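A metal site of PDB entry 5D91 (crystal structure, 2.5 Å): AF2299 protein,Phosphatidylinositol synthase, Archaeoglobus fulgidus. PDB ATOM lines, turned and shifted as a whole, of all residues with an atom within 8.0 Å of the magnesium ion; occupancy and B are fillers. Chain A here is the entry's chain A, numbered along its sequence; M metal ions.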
ATOM      1  N   THR A 163       2.421 -22.846  -0.082  1.00  0.00           N
ATOM      2  CA  THR A 163       2.950 -22.190   1.117  1.00  0.00           C
ATOM      3  C   THR A 163       1.847 -21.721   2.066  1.00  0.00           C
ATOM      4  O   THR A 163       1.889 -21.982   3.280  1.00  0.00           O
ATOM      5  CB  THR A 163       3.828 -20.959   0.758  1.00  0.00           C
ATOM      6  OG1 THR A 163       4.710 -21.293  -0.322  1.00  0.00           O
ATOM      7  CG2 THR A 163       4.654 -20.548   1.964  1.00  0.00           C
ATOM      8  N   VAL A 194       4.162 -29.001   8.174  1.00  0.00           N
ATOM      9  CA  VAL A 194       5.460 -28.367   8.131  1.00  0.00           C
ATOM     10  C   VAL A 194       6.222 -28.860   6.884  1.00  0.00           C
ATOM     11  O   VAL A 194       6.917 -28.088   6.239  1.00  0.00           O
ATOM     12  CB  VAL A 194       6.244 -28.640   9.424  1.00  0.00           C
ATOM     13  CG1 VAL A 194       7.742 -28.728   9.157  1.00  0.00           C
ATOM     14  CG2 VAL A 194       5.938 -27.575  10.447  1.00  0.00           C
ATOM     15  N   SER A 196       5.151 -29.259   4.054  1.00  0.00           N
ATOM     16  CA  SER A 196       4.689 -28.545   2.855  1.00  0.00           C
ATOM     17  C   SER A 196       5.811 -27.640   2.302  1.00  0.00           C
ATOM     18  O   SER A 196       5.815 -27.291   1.120  1.00  0.00           O
ATOM     19  CB  SER A 196       3.431 -27.705   3.129  1.00  0.00           C
ATOM     20  OG  SER A 196       3.725 -26.581   3.947  1.00  0.00           O
ATOM     21  N   ASP A 197       6.753 -27.273   3.183  1.00  0.00           N
ATOM     22  CA  ASP A 197       7.934 -26.484   2.807  1.00  0.00           C
ATOM     23  C   ASP A 197       8.771 -27.245   1.789  1.00  0.00           C
ATOM     24  O   ASP A 197       9.327 -26.646   0.865  1.00  0.00           O
ATOM     25  CB  ASP A 197       8.777 -26.088   4.032  1.00  0.00           C
ATOM     26  CG  ASP A 197       8.356 -24.729   4.638  1.00  0.00           C
ATOM     27  OD1 ASP A 197       9.253 -23.860   4.833  1.00  0.00           O
ATOM     28  OD2 ASP A 197       7.159 -24.552   4.938  1.00  0.00           O
ATOM     29  N   ILE A 198       8.941 -28.546   1.979  1.00  0.00           N
ATOM     30  CA  ILE A 198       9.752 -29.302   1.035  1.00  0.00           C
ATOM     31  C   ILE A 198       9.054 -29.362  -0.321  1.00  0.00           C
ATOM     32  O   ILE A 198       9.702 -29.265  -1.377  1.00  0.00           O
ATOM     33  CB  ILE A 198      10.014 -30.745   1.533  1.00  0.00           C
ATOM     34  CG1 ILE A 198      10.678 -30.726   2.914  1.00  0.00           C
ATOM     35  CG2 ILE A 198      10.900 -31.510   0.588  1.00  0.00           C
ATOM     36  CD1 ILE A 198      11.019 -32.099   3.433  1.00  0.00           C
ATOM     37  N   ASP A 200       6.873 -26.887  -1.560  1.00  0.00           N
ATOM     38  CA  ASP A 200       6.974 -25.598  -2.277  1.00  0.00           C
ATOM     39  C   ASP A 200       8.397 -25.328  -2.786  1.00  0.00           C
ATOM     40  O   ASP A 200       8.588 -24.666  -3.806  1.00  0.00           O
ATOM     41  CB  ASP A 200       6.450 -24.416  -1.428  1.00  0.00           C
ATOM     42  CG  ASP A 200       7.111 -24.309  -0.053  1.00  0.00           C
ATOM     43  OD1 ASP A 200       8.358 -24.353   0.014  1.00  0.00           O
ATOM     44  OD2 ASP A 200       6.374 -24.156   0.952  1.00  0.00           O
ATOM     45  N   GLY A 201       9.387 -25.883  -2.103  1.00  0.00           N
ATOM     46  CA  GLY A 201      10.776 -25.748  -2.511  1.00  0.00           C
ATOM     47  C   GLY A 201      11.004 -26.486  -3.819  1.00  0.00           C
ATOM     48  O   GLY A 201      11.677 -25.996  -4.743  1.00  0.00           O
ATOM     49  N   GLY A 214       8.773 -14.597  -3.728  1.00  0.00           N
ATOM     50  CA  GLY A 214       8.794 -15.948  -3.211  1.00  0.00           C
ATOM     51  C   GLY A 214       9.554 -16.010  -1.912  1.00  0.00           C
ATOM     52  O   GLY A 214       9.041 -16.505  -0.913  1.00  0.00           O
ATOM     53  N   ALA A 215      10.751 -15.438  -1.924  1.00  0.00           N
ATOM     54  CA  ALA A 215      11.581 -15.359  -0.723  1.00  0.00           C
ATOM     55  C   ALA A 215      10.848 -14.610   0.404  1.00  0.00           C
ATOM     56  O   ALA A 215      10.835 -15.061   1.551  1.00  0.00           O
ATOM     57  CB  ALA A 215      12.901 -14.683  -1.059  1.00  0.00           C
ATOM     58  N   LEU A 217       7.626 -14.173   0.908  1.00  0.00           N
ATOM     59  CA  LEU A 217       6.501 -14.933   1.428  1.00  0.00           C
ATOM     60  C   LEU A 217       6.926 -16.113   2.325  1.00  0.00           C
ATOM     61  O   LEU A 217       6.399 -16.286   3.424  1.00  0.00           O
ATOM     62  CB  LEU A 217       5.634 -15.379   0.269  1.00  0.00           C
ATOM     63  CG  LEU A 217       4.254 -15.958   0.562  1.00  0.00           C
ATOM     64  CD1 LEU A 217       3.407 -14.964   1.357  1.00  0.00           C
ATOM     65  CD2 LEU A 217       3.575 -16.256  -0.764  1.00  0.00           C
ATOM     66  N   ASP A 218       7.908 -16.896   1.861  1.00  0.00           N
ATOM     67  CA  ASP A 218       8.511 -17.959   2.663  1.00  0.00           C
ATOM     68  C   ASP A 218       9.001 -17.490   4.040  1.00  0.00           C
ATOM     69  O   ASP A 218       8.671 -18.097   5.047  1.00  0.00           O
ATOM     70  CB  ASP A 218       9.668 -18.614   1.883  1.00  0.00           C
ATOM     71  CG  ASP A 218      10.463 -19.609   2.722  1.00  0.00           C
ATOM     72  OD1 ASP A 218       9.995 -20.754   2.932  1.00  0.00           O
ATOM     73  OD2 ASP A 218      11.586 -19.248   3.157  1.00  0.00           O
ATOM     74  N   SER A 219       9.792 -16.406   4.080  1.00  0.00           N
ATOM     75  CA  SER A 219      10.211 -15.830   5.360  1.00  0.00           C
ATOM     76  C   SER A 219       9.036 -15.424   6.230  1.00  0.00           C
ATOM     77  O   SER A 219       8.984 -15.741   7.418  1.00  0.00           O
ATOM     78  CB  SER A 219      11.107 -14.614   5.191  1.00  0.00           C
ATOM     79  OG  SER A 219      12.276 -14.924   4.501  1.00  0.00           O
ATOM     80  N   TYR A 220       8.107 -14.668   5.650  1.00  0.00           N
ATOM     81  CA  TYR A 220       6.987 -14.139   6.416  1.00  0.00           C
ATOM     82  C   TYR A 220       6.079 -15.232   6.994  1.00  0.00           C
ATOM     83  O   TYR A 220       5.777 -15.214   8.192  1.00  0.00           O
ATOM     84  CB  TYR A 220       6.167 -13.177   5.558  1.00  0.00           C
ATOM     85  CG  TYR A 220       5.356 -12.234   6.384  1.00  0.00           C
ATOM     86  CD1 TYR A 220       5.977 -11.233   7.101  1.00  0.00           C
ATOM     87  CD2 TYR A 220       3.971 -12.321   6.436  1.00  0.00           C
ATOM     88  CE1 TYR A 220       5.246 -10.336   7.861  1.00  0.00           C
ATOM     89  CE2 TYR A 220       3.227 -11.431   7.197  1.00  0.00           C
ATOM     90  CZ  TYR A 220       3.870 -10.441   7.912  1.00  0.00           C
ATOM     91  OH  TYR A 220       3.169  -9.541   8.683  1.00  0.00           O
ATOM     92  N   LEU A 221       5.623 -16.144   6.146  1.00  0.00           N
ATOM     93  CA  LEU A 221       4.712 -17.196   6.582  1.00  0.00           C
ATOM     94  C   LEU A 221       5.398 -18.132   7.576  1.00  0.00           C
ATOM     95  O   LEU A 221       4.738 -18.743   8.419  1.00  0.00           O
ATOM     96  CB  LEU A 221       4.135 -17.965   5.380  1.00  0.00           C
ATOM     97  CG  LEU A 221       3.203 -17.080   4.525  1.00  0.00           C
ATOM     98  CD1 LEU A 221       2.414 -17.885   3.494  1.00  0.00           C
ATOM     99  CD2 LEU A 221       2.226 -16.231   5.374  1.00  0.00           C
ATOM    100  N   ASP A 222       6.727 -18.205   7.520  1.00  0.00           N
ATOM    101  CA  ASP A 222       7.469 -19.022   8.474  1.00  0.00           C
ATOM    102  C   ASP A 222       7.359 -18.365   9.847  1.00  0.00           C
ATOM    103  O   ASP A 222       7.161 -19.063  10.846  1.00  0.00           O
ATOM    104  CB  ASP A 222       8.940 -19.181   8.067  1.00  0.00           C
ATOM    105  CG  ASP A 222       9.148 -20.329   7.082  1.00  0.00           C
ATOM    106  OD1 ASP A 222       8.151 -21.016   6.771  1.00  0.00           O
ATOM    107  OD2 ASP A 222      10.283 -20.546   6.589  1.00  0.00           O
ATOM    108  N   ARG A 223       7.513 -17.033   9.879  1.00  0.00           N
ATOM    109  CA  ARG A 223       7.313 -16.255  11.107  1.00  0.00           C
ATOM    110  C   ARG A 223       5.918 -16.438  11.700  1.00  0.00           C
ATOM    111  O   ARG A 223       5.777 -16.632  12.914  1.00  0.00           O
ATOM    112  CB  ARG A 223       7.567 -14.758  10.904  1.00  0.00           C
ATOM    113  CG  ARG A 223       9.024 -14.343  10.977  1.00  0.00           C
ATOM    114  CD  ARG A 223       9.713 -14.915  12.218  1.00  0.00           C
ATOM    115  NE  ARG A 223       8.935 -14.651  13.435  1.00  0.00           N
ATOM    116  CZ  ARG A 223       9.086 -15.323  14.582  1.00  0.00           C
ATOM    117  NH1 ARG A 223       8.324 -15.016  15.620  1.00  0.00           N
ATOM    118  NH2 ARG A 223       9.966 -16.316  14.687  1.00  0.00           N
ATOM    119  N   ARG A 281      15.981 -21.948  13.232  1.00  0.00           N
ATOM    120  CA  ARG A 281      14.530 -21.979  13.286  1.00  0.00           C
ATOM    121  C   ARG A 281      13.912 -23.380  13.251  1.00  0.00           C
ATOM    122  O   ARG A 281      13.070 -23.690  14.089  1.00  0.00           O
ATOM    123  CB  ARG A 281      13.962 -21.153  12.135  1.00  0.00           C
ATOM    124  CG  ARG A 281      12.463 -21.081  12.145  1.00  0.00           C
ATOM    125  CD  ARG A 281      11.878 -21.420  10.780  1.00  0.00           C
ATOM    126  NE  ARG A 281      10.429 -21.550  10.846  1.00  0.00           N
ATOM    127  CZ  ARG A 281       9.718 -22.417  10.133  1.00  0.00           C
ATOM    128  NH1 ARG A 281      10.335 -23.229   9.273  1.00  0.00           N
ATOM    129  NH2 ARG A 281       8.394 -22.468  10.258  1.00  0.00           N
HETATM  130 MG    MG M   1      10.382 -21.942   4.686  1.00  0.00          MG
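The guanidinium group (NH2) of Arg 281 lies within salt-bridge range of the side-chain carboxylate (OD1) of Asp 222 (3.8 Å). O of Asp 197 sits close to OD1 of Asp 200, at 2.6 Å.
Within 4 Å of the magnesium ion: Asp 197, Asp 218 and Asp 222. The nearest printed residue that does not touch the magnesium ion is Arg 281 (4.8 Å).
The magnesium ion is bound by the side-chain carboxylate (OD1) of Asp 218 (2.2 Å). The magnesium ion is bound by OD1 of Asp 197, 2.2 Å away. OD2 of Asp 222 is bound to the magnesium ion (2.4 Å). The magnesium ion has three donor atoms within binding distance.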
